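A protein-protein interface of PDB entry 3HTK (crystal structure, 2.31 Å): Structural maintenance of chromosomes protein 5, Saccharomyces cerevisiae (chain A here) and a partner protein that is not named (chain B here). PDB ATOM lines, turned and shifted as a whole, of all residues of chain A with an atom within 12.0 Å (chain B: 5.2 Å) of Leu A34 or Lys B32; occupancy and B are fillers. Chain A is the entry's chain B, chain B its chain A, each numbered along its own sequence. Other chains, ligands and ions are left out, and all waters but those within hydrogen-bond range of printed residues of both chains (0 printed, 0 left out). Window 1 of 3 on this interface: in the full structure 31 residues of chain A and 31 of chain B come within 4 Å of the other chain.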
ATOM      1  N   SER A  25       3.356  -8.176  28.506  1.00  0.00           N
ATOM      2  CA  SER A  25       3.116  -8.660  27.155  1.00  0.00           C
ATOM      3  C   SER A  25       4.444  -8.665  26.381  1.00  0.00           C
ATOM      4  O   SER A  25       4.751  -9.625  25.677  1.00  0.00           O
ATOM      5  CB  SER A  25       2.111  -7.756  26.451  1.00  0.00           C
ATOM      6  OG  SER A  25       1.772  -8.277  25.184  1.00  0.00           O
ATOM      7  N   LYS A  26       5.226  -7.596  26.520  1.00  0.00           N
ATOM      8  CA  LYS A  26       6.533  -7.493  25.859  1.00  0.00           C
ATOM      9  C   LYS A  26       7.450  -8.621  26.347  1.00  0.00           C
ATOM     10  O   LYS A  26       8.141  -9.270  25.564  1.00  0.00           O
ATOM     11  CB  LYS A  26       7.187  -6.148  26.175  1.00  0.00           C
ATOM     12  CG  LYS A  26       6.533  -4.958  25.512  1.00  0.00           C
ATOM     13  CD  LYS A  26       6.732  -4.995  24.004  1.00  0.00           C
ATOM     14  CE  LYS A  26       6.205  -3.717  23.342  1.00  0.00           C
ATOM     15  NZ  LYS A  26       6.441  -3.721  21.861  1.00  0.00           N
ATOM     16  N   MET A  27       7.443  -8.837  27.654  1.00  0.00           N
ATOM     17  CA  MET A  27       8.237  -9.878  28.283  1.00  0.00           C
ATOM     18  C   MET A  27       7.997 -11.250  27.631  1.00  0.00           C
ATOM     19  O   MET A  27       8.941 -11.982  27.344  1.00  0.00           O
ATOM     20  CB  MET A  27       7.895  -9.926  29.776  1.00  0.00           C
ATOM     21  CG  MET A  27       8.563 -11.032  30.535  1.00  0.00           C
ATOM     22  SD  MET A  27       8.003 -11.063  32.241  1.00  0.00           S
ATOM     23  CE  MET A  27       6.589 -12.139  32.085  1.00  0.00           C
ATOM     24  N   ALA A  28       6.732 -11.598  27.418  1.00  0.00           N
ATOM     25  CA  ALA A  28       6.376 -12.873  26.791  1.00  0.00           C
ATOM     26  C   ALA A  28       6.869 -12.919  25.340  1.00  0.00           C
ATOM     27  O   ALA A  28       7.324 -13.958  24.859  1.00  0.00           O
ATOM     28  CB  ALA A  28       4.867 -13.069  26.828  1.00  0.00           C
ATOM     29  N   SER A  29       6.757 -11.787  24.653  1.00  0.00           N
ATOM     30  CA  SER A  29       7.194 -11.671  23.268  1.00  0.00           C
ATOM     31  C   SER A  29       8.707 -11.868  23.242  1.00  0.00           C
ATOM     32  O   SER A  29       9.251 -12.551  22.367  1.00  0.00           O
ATOM     33  CB  SER A  29       6.854 -10.281  22.739  1.00  0.00           C
ATOM     34  OG  SER A  29       7.458 -10.036  21.480  1.00  0.00           O
ATOM     35  N   SER A  30       9.365 -11.252  24.219  1.00  0.00           N
ATOM     36  CA  SER A  30      10.807 -11.311  24.372  1.00  0.00           C
ATOM     37  C   SER A  30      11.247 -12.739  24.636  1.00  0.00           C
ATOM     38  O   SER A  30      12.304 -13.170  24.173  1.00  0.00           O
ATOM     39  CB  SER A  30      11.240 -10.406  25.528  1.00  0.00           C
ATOM     40  OG  SER A  30      12.642 -10.402  25.676  1.00  0.00           O
ATOM     41  N   MET A  31      10.440 -13.468  25.393  1.00  0.00           N
ATOM     42  CA  MET A  31      10.744 -14.851  25.696  1.00  0.00           C
ATOM     43  C   MET A  31      10.756 -15.652  24.386  1.00  0.00           C
ATOM     44  O   MET A  31      11.716 -16.380  24.090  1.00  0.00           O
ATOM     45  CB  MET A  31       9.695 -15.422  26.641  1.00  0.00           C
ATOM     46  CG  MET A  31       9.968 -16.843  27.049  1.00  0.00           C
ATOM     47  SD  MET A  31      11.548 -16.987  27.891  1.00  0.00           S
ATOM     48  CE  MET A  31      11.036 -17.152  29.559  1.00  0.00           C
ATOM     49  N   LYS A  32       9.688 -15.501  23.602  1.00  0.00           N
ATOM     50  CA  LYS A  32       9.568 -16.186  22.325  1.00  0.00           C
ATOM     51  C   LYS A  32      10.805 -15.950  21.454  1.00  0.00           C
ATOM     52  O   LYS A  32      11.300 -16.873  20.826  1.00  0.00           O
ATOM     53  CB  LYS A  32       8.332 -15.704  21.568  1.00  0.00           C
ATOM     54  CG  LYS A  32       8.074 -16.485  20.295  1.00  0.00           C
ATOM     55  CD  LYS A  32       7.146 -15.721  19.366  1.00  0.00           C
ATOM     56  CE  LYS A  32       7.011 -16.421  18.006  1.00  0.00           C
ATOM     57  NZ  LYS A  32       6.179 -15.629  17.046  1.00  0.00           N
ATOM     58  N   SER A  33      11.288 -14.714  21.412  1.00  0.00           N
ATOM     59  CA  SER A  33      12.471 -14.396  20.618  1.00  0.00           C
ATOM     60  C   SER A  33      13.695 -15.097  21.191  1.00  0.00           C
ATOM     61  O   SER A  33      14.605 -15.481  20.456  1.00  0.00           O
ATOM     62  CB  SER A  33      12.732 -12.891  20.594  1.00  0.00           C
ATOM     63  OG  SER A  33      12.064 -12.278  19.510  1.00  0.00           O
ATOM     64  N   LEU A  34      13.705 -15.248  22.509  1.00  0.00           N
ATOM     65  CA  LEU A  34      14.810 -15.891  23.188  1.00  0.00           C
ATOM     66  C   LEU A  34      14.806 -17.380  22.817  1.00  0.00           C
ATOM     67  O   LEU A  34      15.849 -17.937  22.490  1.00  0.00           O
ATOM     68  CB  LEU A  34      14.683 -15.678  24.707  1.00  0.00           C
ATOM     69  CG  LEU A  34      15.849 -16.048  25.637  1.00  0.00           C
ATOM     70  CD1 LEU A  34      16.000 -17.542  25.693  1.00  0.00           C
ATOM     71  CD2 LEU A  34      17.141 -15.404  25.155  1.00  0.00           C
ATOM     72  N   LYS A  35      13.636 -18.012  22.863  1.00  0.00           N
ATOM     73  CA  LYS A  35      13.506 -19.417  22.496  1.00  0.00           C
ATOM     74  C   LYS A  35      13.999 -19.626  21.068  1.00  0.00           C
ATOM     75  O   LYS A  35      14.594 -20.656  20.775  1.00  0.00           O
ATOM     76  CB  LYS A  35      12.054 -19.884  22.568  1.00  0.00           C
ATOM     77  CG  LYS A  35      11.397 -19.685  23.900  1.00  0.00           C
ATOM     78  CD  LYS A  35       9.902 -20.012  23.837  1.00  0.00           C
ATOM     79  CE  LYS A  35       9.622 -21.515  23.883  1.00  0.00           C
ATOM     80  NZ  LYS A  35       9.966 -22.248  22.641  1.00  0.00           N
ATOM     81  N   ASN A  36      13.741 -18.663  20.182  1.00  0.00           N
ATOM     82  CA  ASN A  36      14.191 -18.776  18.795  1.00  0.00           C
ATOM     83  C   ASN A  36      15.701 -18.747  18.701  1.00  0.00           C
ATOM     84  O   ASN A  36      16.273 -19.521  17.949  1.00  0.00           O
ATOM     85  CB  ASN A  36      13.627 -17.666  17.906  1.00  0.00           C
ATOM     86  CG  ASN A  36      12.161 -17.846  17.618  1.00  0.00           C
ATOM     87  OD1 ASN A  36      11.689 -18.972  17.448  1.00  0.00           O
ATOM     88  ND2 ASN A  36      11.422 -16.734  17.553  1.00  0.00           N
ATOM     89  N   CYS A  37      16.342 -17.842  19.438  1.00  0.00           N
ATOM     90  CA  CYS A  37      17.800 -17.763  19.439  1.00  0.00           C
ATOM     91  C   CYS A  37      18.358 -19.058  19.994  1.00  0.00           C
ATOM     92  O   CYS A  37      19.340 -19.594  19.468  1.00  0.00           O
ATOM     93  CB  CYS A  37      18.300 -16.623  20.324  1.00  0.00           C
ATOM     94  SG  CYS A  37      18.091 -14.981  19.660  1.00  0.00           S
ATOM     95  N   GLN A  38      17.739 -19.550  21.070  1.00  0.00           N
ATOM     96  CA  GLN A  38      18.209 -20.779  21.687  1.00  0.00           C
ATOM     97  C   GLN A  38      18.108 -21.910  20.671  1.00  0.00           C
ATOM     98  O   GLN A  38      19.026 -22.704  20.531  1.00  0.00           O
ATOM     99  CB  GLN A  38      17.386 -21.106  22.943  1.00  0.00           C
ATOM    100  CG  GLN A  38      17.613 -22.509  23.489  1.00  0.00           C
ATOM    101  CD  GLN A  38      16.336 -23.148  24.028  1.00  0.00           C
ATOM    102  OE1 GLN A  38      15.278 -23.060  23.409  1.00  0.00           O
ATOM    103  NE2 GLN A  38      16.441 -23.816  25.168  1.00  0.00           N
ATOM    104  N   LYS A  39      16.995 -21.968  19.951  1.00  0.00           N
ATOM    105  CA  LYS A  39      16.793 -23.013  18.958  1.00  0.00           C
ATOM    106  C   LYS A  39      17.803 -22.914  17.808  1.00  0.00           C
ATOM    107  O   LYS A  39      18.379 -23.916  17.393  1.00  0.00           O
ATOM    108  CB  LYS A  39      15.361 -22.942  18.420  1.00  0.00           C
ATOM    109  CG  LYS A  39      14.961 -24.099  17.506  1.00  0.00           C
ATOM    110  CD  LYS A  39      13.478 -24.039  17.188  1.00  0.00           C
ATOM    111  CE  LYS A  39      13.047 -25.155  16.240  1.00  0.00           C
ATOM    112  NZ  LYS A  39      13.228 -26.520  16.814  1.00  0.00           N
ATOM    113  N   GLU A  40      18.020 -21.703  17.311  1.00  0.00           N
ATOM    114  CA  GLU A  40      18.960 -21.458  16.224  1.00  0.00           C
ATOM    115  C   GLU A  40      20.415 -21.746  16.617  1.00  0.00           C
ATOM    116  O   GLU A  40      21.231 -22.141  15.769  1.00  0.00           O
ATOM    117  CB  GLU A  40      18.835 -20.012  15.760  1.00  0.00           C
ATOM    118  CG  GLU A  40      17.492 -19.696  15.124  1.00  0.00           C
ATOM    119  CD  GLU A  40      17.273 -18.211  14.925  1.00  0.00           C
ATOM    120  OE1 GLU A  40      18.179 -17.548  14.378  1.00  0.00           O
ATOM    121  OE2 GLU A  40      16.188 -17.708  15.312  1.00  0.00           O
ATOM    122  N   LEU A  41      20.730 -21.541  17.893  1.00  0.00           N
ATOM    123  CA  LEU A  41      22.072 -21.780  18.401  1.00  0.00           C
ATOM    124  C   LEU A  41      22.384 -23.269  18.423  1.00  0.00           C
ATOM    125  O   LEU A  41      23.450 -23.678  17.955  1.00  0.00           O
ATOM    126  CB  LEU A  41      22.232 -21.224  19.815  1.00  0.00           C
ATOM    127  CG  LEU A  41      23.570 -21.556  20.460  1.00  0.00           C
ATOM    128  CD1 LEU A  41      24.714 -20.901  19.654  1.00  0.00           C
ATOM    129  CD2 LEU A  41      23.560 -21.072  21.915  1.00  0.00           C
ATOM    130  N   ILE A  42      21.471 -24.073  18.971  1.00  0.00           N
ATOM    131  CA  ILE A  42      21.683 -25.516  19.018  1.00  0.00           C
ATOM    132  C   ILE A  42      21.749 -26.121  17.612  1.00  0.00           C
ATOM    133  O   ILE A  42      22.511 -27.062  17.375  1.00  0.00           O
ATOM    134  CB  ILE A  42      20.580 -26.246  19.855  1.00  0.00           C
ATOM    135  CG1 ILE A  42      20.920 -27.732  19.994  1.00  0.00           C
ATOM    136  CG2 ILE A  42      19.235 -26.099  19.210  1.00  0.00           C
ATOM    137  CD1 ILE A  42      22.196 -28.002  20.751  1.00  0.00           C
ATOM    138  N   SER A  43      20.966 -25.576  16.681  1.00  0.00           N
ATOM    139  CA  SER A  43      20.965 -26.054  15.294  1.00  0.00           C
ATOM    140  C   SER A  43      22.321 -25.816  14.649  1.00  0.00           C
ATOM    141  O   SER A  43      22.917 -26.718  14.078  1.00  0.00           O
ATOM    142  CB  SER A  43      19.933 -25.307  14.452  1.00  0.00           C
ATOM    143  OG  SER A  43      18.615 -25.696  14.768  1.00  0.00           O
ATOM    144  N   THR A  44      22.792 -24.580  14.721  1.00  0.00           N
ATOM    145  CA  THR A  44      24.056 -24.245  14.111  1.00  0.00           C
ATOM    146  C   THR A  44      25.164 -25.085  14.749  1.00  0.00           C
ATOM    147  O   THR A  44      26.059 -25.570  14.054  1.00  0.00           O
ATOM    148  CB  THR A  44      24.317 -22.704  14.208  1.00  0.00           C
ATOM    149  OG1 THR A  44      25.676 -22.413  13.881  1.00  0.00           O
ATOM    150  CG2 THR A  44      24.023 -22.193  15.589  1.00  0.00           C
ATOM    151  N   GLN A  45      25.072 -25.308  16.054  1.00  0.00           N
ATOM    152  CA  GLN A  45      26.081 -26.091  16.740  1.00  0.00           C
ATOM    153  C   GLN A  45      26.123 -27.546  16.304  1.00  0.00           C
ATOM    154  O   GLN A  45      27.196 -28.159  16.328  1.00  0.00           O
ATOM    155  CB  GLN A  45      25.879 -26.034  18.244  1.00  0.00           C
ATOM    156  CG  GLN A  45      26.148 -24.698  18.840  1.00  0.00           C
ATOM    157  CD  GLN A  45      25.690 -24.635  20.267  1.00  0.00           C
ATOM    158  OE1 GLN A  45      24.601 -25.100  20.586  1.00  0.00           O
ATOM    159  NE2 GLN A  45      26.505 -24.053  21.135  1.00  0.00           N
ATOM    160  N   PHE B  28      22.223 -14.881  21.203  1.00  0.00           N
ATOM    161  CA  PHE B  28      21.432 -15.484  22.266  1.00  0.00           C
ATOM    162  C   PHE B  28      21.639 -14.771  23.605  1.00  0.00           C
ATOM    163  O   PHE B  28      20.685 -14.527  24.332  1.00  0.00           O
ATOM    164  CB  PHE B  28      21.803 -16.954  22.444  1.00  0.00           C
ATOM    165  CG  PHE B  28      21.241 -17.567  23.692  1.00  0.00           C
ATOM    166  CD1 PHE B  28      19.949 -18.073  23.713  1.00  0.00           C
ATOM    167  CD2 PHE B  28      22.005 -17.622  24.858  1.00  0.00           C
ATOM    168  CE1 PHE B  28      19.413 -18.635  24.877  1.00  0.00           C
ATOM    169  CE2 PHE B  28      21.484 -18.174  26.023  1.00  0.00           C
ATOM    170  CZ  PHE B  28      20.174 -18.688  26.033  1.00  0.00           C
ATOM    171  N   LEU B  29      22.885 -14.460  23.943  1.00  0.00           N
ATOM    172  CA  LEU B  29      23.149 -13.779  25.198  1.00  0.00           C
ATOM    173  C   LEU B  29      22.570 -12.376  25.145  1.00  0.00           C
ATOM    174  O   LEU B  29      22.187 -11.818  26.171  1.00  0.00           O
ATOM    175  CB  LEU B  29      24.651 -13.724  25.477  1.00  0.00           C
ATOM    176  CG  LEU B  29      25.317 -15.089  25.694  1.00  0.00           C
ATOM    177  CD1 LEU B  29      26.806 -14.884  25.993  1.00  0.00           C
ATOM    178  CD2 LEU B  29      24.638 -15.837  26.851  1.00  0.00           C
ATOM    179  N   LYS B  30      22.499 -11.811  23.943  1.00  0.00           N
ATOM    180  CA  LYS B  30      21.944 -10.468  23.763  1.00  0.00           C
ATOM    181  C   LYS B  30      20.452 -10.517  24.085  1.00  0.00           C
ATOM    182  O   LYS B  30      19.936  -9.674  24.816  1.00  0.00           O
ATOM    183  CB  LYS B  30      22.120  -9.992  22.316  1.00  0.00           C
ATOM    184  CG  LYS B  30      22.608  -8.559  22.186  1.00  0.00           C
ATOM    185  CD  LYS B  30      24.117  -8.453  22.435  1.00  0.00           C
ATOM    186  CE  LYS B  30      24.919  -8.750  21.156  1.00  0.00           C
ATOM    187  NZ  LYS B  30      26.403  -8.611  21.313  1.00  0.00           N
ATOM    188  N   ALA B  31      19.759 -11.510  23.540  1.00  0.00           N
ATOM    189  CA  ALA B  31      18.328 -11.634  23.775  1.00  0.00           C
ATOM    190  C   ALA B  31      18.051 -11.818  25.270  1.00  0.00           C
ATOM    191  O   ALA B  31      17.096 -11.258  25.798  1.00  0.00           O
ATOM    192  CB  ALA B  31      17.759 -12.802  22.972  1.00  0.00           C
ATOM    193  N   LYS B  32      18.894 -12.592  25.947  1.00  0.00           N
ATOM    194  CA  LYS B  32      18.741 -12.838  27.381  1.00  0.00           C
ATOM    195  C   LYS B  32      18.786 -11.488  28.094  1.00  0.00           C
ATOM    196  O   LYS B  32      18.003 -11.221  29.014  1.00  0.00           O
ATOM    197  CB  LYS B  32      19.887 -13.712  27.881  1.00  0.00           C
ATOM    198  CG  LYS B  32      19.545 -14.678  28.987  1.00  0.00           C
ATOM    199  CD  LYS B  32      20.697 -15.667  29.172  1.00  0.00           C
ATOM    200  CE  LYS B  32      20.253 -16.976  29.823  1.00  0.00           C
ATOM    201  NZ  LYS B  32      19.769 -16.813  31.228  1.00  0.00           N
ATOM    202  N   GLU B  33      19.717 -10.645  27.662  1.00  0.00           N
ATOM    203  CA  GLU B  33      19.867  -9.327  28.240  1.00  0.00           C
ATOM    204  C   GLU B  33      18.651  -8.439  27.995  1.00  0.00           C
ATOM    205  O   GLU B  33      18.288  -7.637  28.852  1.00  0.00           O
ATOM    206  CB  GLU B  33      21.138  -8.668  27.703  1.00  0.00           C
ATOM    207  CG  GLU B  33      22.386  -9.143  28.434  1.00  0.00           C
ATOM    208  CD  GLU B  33      23.678  -8.697  27.775  1.00  0.00           C
ATOM    209  OE1 GLU B  33      24.742  -8.820  28.429  1.00  0.00           O
ATOM    210  OE2 GLU B  33      23.631  -8.235  26.610  1.00  0.00           O
ATOM    211  N   LYS B  34      18.014  -8.585  26.839  1.00  0.00           N
ATOM    212  CA  LYS B  34      16.838  -7.782  26.528  1.00  0.00           C
ATOM    213  C   LYS B  34      15.695  -8.075  27.509  1.00  0.00           C
ATOM    214  O   LYS B  34      15.038  -7.159  28.022  1.00  0.00           O
ATOM    215  CB  LYS B  34      16.349  -8.068  25.102  1.00  0.00           C
ATOM    216  CG  LYS B  34      17.369  -7.832  23.997  1.00  0.00           C
ATOM    217  CD  LYS B  34      17.802  -6.373  23.920  1.00  0.00           C
ATOM    218  CE  LYS B  34      18.581  -6.087  22.633  1.00  0.00           C
ATOM    219  NZ  LYS B  34      19.836  -6.884  22.501  1.00  0.00           N
ATOM    220  N   ILE B  35      15.453  -9.356  27.762  1.00  0.00           N
ATOM    221  CA  ILE B  35      14.375  -9.741  28.649  1.00  0.00           C
ATOM    222  C   ILE B  35      14.700  -9.300  30.078  1.00  0.00           C
ATOM    223  O   ILE B  35      13.807  -8.887  30.812  1.00  0.00           O
ATOM    224  CB  ILE B  35      14.095 -11.270  28.540  1.00  0.00           C
ATOM    225  CG1 ILE B  35      12.714 -11.607  29.114  1.00  0.00           C
ATOM    226  CG2 ILE B  35      15.172 -12.048  29.244  1.00  0.00           C
ATOM    227  CD1 ILE B  35      12.284 -13.068  28.896  1.00  0.00           C
ATOM    228  N   ASN B  36      15.976  -9.347  30.471  1.00  0.00           N
ATOM    229  CA  ASN B  36      16.342  -8.902  31.814  1.00  0.00           C
ATOM    230  C   ASN B  36      16.081  -7.397  31.954  1.00  0.00           C
ATOM    231  O   ASN B  36      15.815  -6.905  33.052  1.00  0.00           O
ATOM    232  CB  ASN B  36      17.811  -9.216  32.138  1.00  0.00           C
ATOM    233  CG  ASN B  36      18.023 -10.666  32.599  1.00  0.00           C
ATOM    234  OD1 ASN B  36      17.286 -11.188  33.439  1.00  0.00           O
ATOM    235  ND2 ASN B  36      19.048 -11.314  32.055  1.00  0.00           N
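The backbone carbonyl oxygen (O) of Lys B32 is in hydrogen-bond range of the side-chain amide nitrogen (ND2) of Asn B36, at 3.2 Å. The backbone carbonyl oxygen of Ser A33 is in hydrogen-bond range of the side-chain sulfur of Cys A37, 3.6 Å away.
Among the printed residues, pairs that only touch across the chains: Met A27 with Ile B35 (3.8 Å), Ser A30 with Ile B35 (3.3 Å), Met A31 with Ile B35 (3.97 Å), Leu A34 with Phe B28 (3.7 Å), Leu A34 with Ala B31 (3.5 Å), Leu A34 with Lys B32 (3.4 Å), Cys A37 with Phe B28 (3.9 Å), Cys A37 with Ala B31 (3.98 Å) and Gln A38 with Phe B28 (3.7 Å).
Of the printed residues of chain B, Leu A34 touches Phe B28, Ala B31 and Lys B32. No residue of chain A comes within 4 Å of Leu B29. No residue of chain A comes within 4 Å of Glu B33. No residue of chain A comes within 4 Å of Lys B34. Of chain A, only Met A27 (3.8 Å), Ser A30 (3.3 Å) and Met A31 (3.97 Å) come within 4 Å of Ile B35. No residue of chain A comes within 4 Å of Asn B36. Printed residues of chain B within 4 Å of Met A27: Ile B35. Of the printed residues of chain B, Ser A30 touches Ile B35. Of the printed residues of chain B, Gln A38 touches Phe B28. The nearest printed residue of chain B that does not touch Leu A34 is Ile B35 (5.4 Å). The nearest residue of chain A that does not touch Lys B32 is Ser A30 (6.4 Å).
Hydrophobic or aromatic side chains of chain A within 4 Å of the printed part of chain B: Leu A34. Of the 9 printed residues of chain B, 4 touch a printed residue of chain A. Printed residues of chain B that touch a printed residue of chain A: Phe B28, Ala B31, Lys B32 and Ile B35. Along chain B the printed residues that touch a printed residue of chain A span positions 28 to 35. Among the printed residues, no Asp or Glu carboxylate lies within 4 Å of a Lys or Arg side-chain nitrogen of the other chain.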
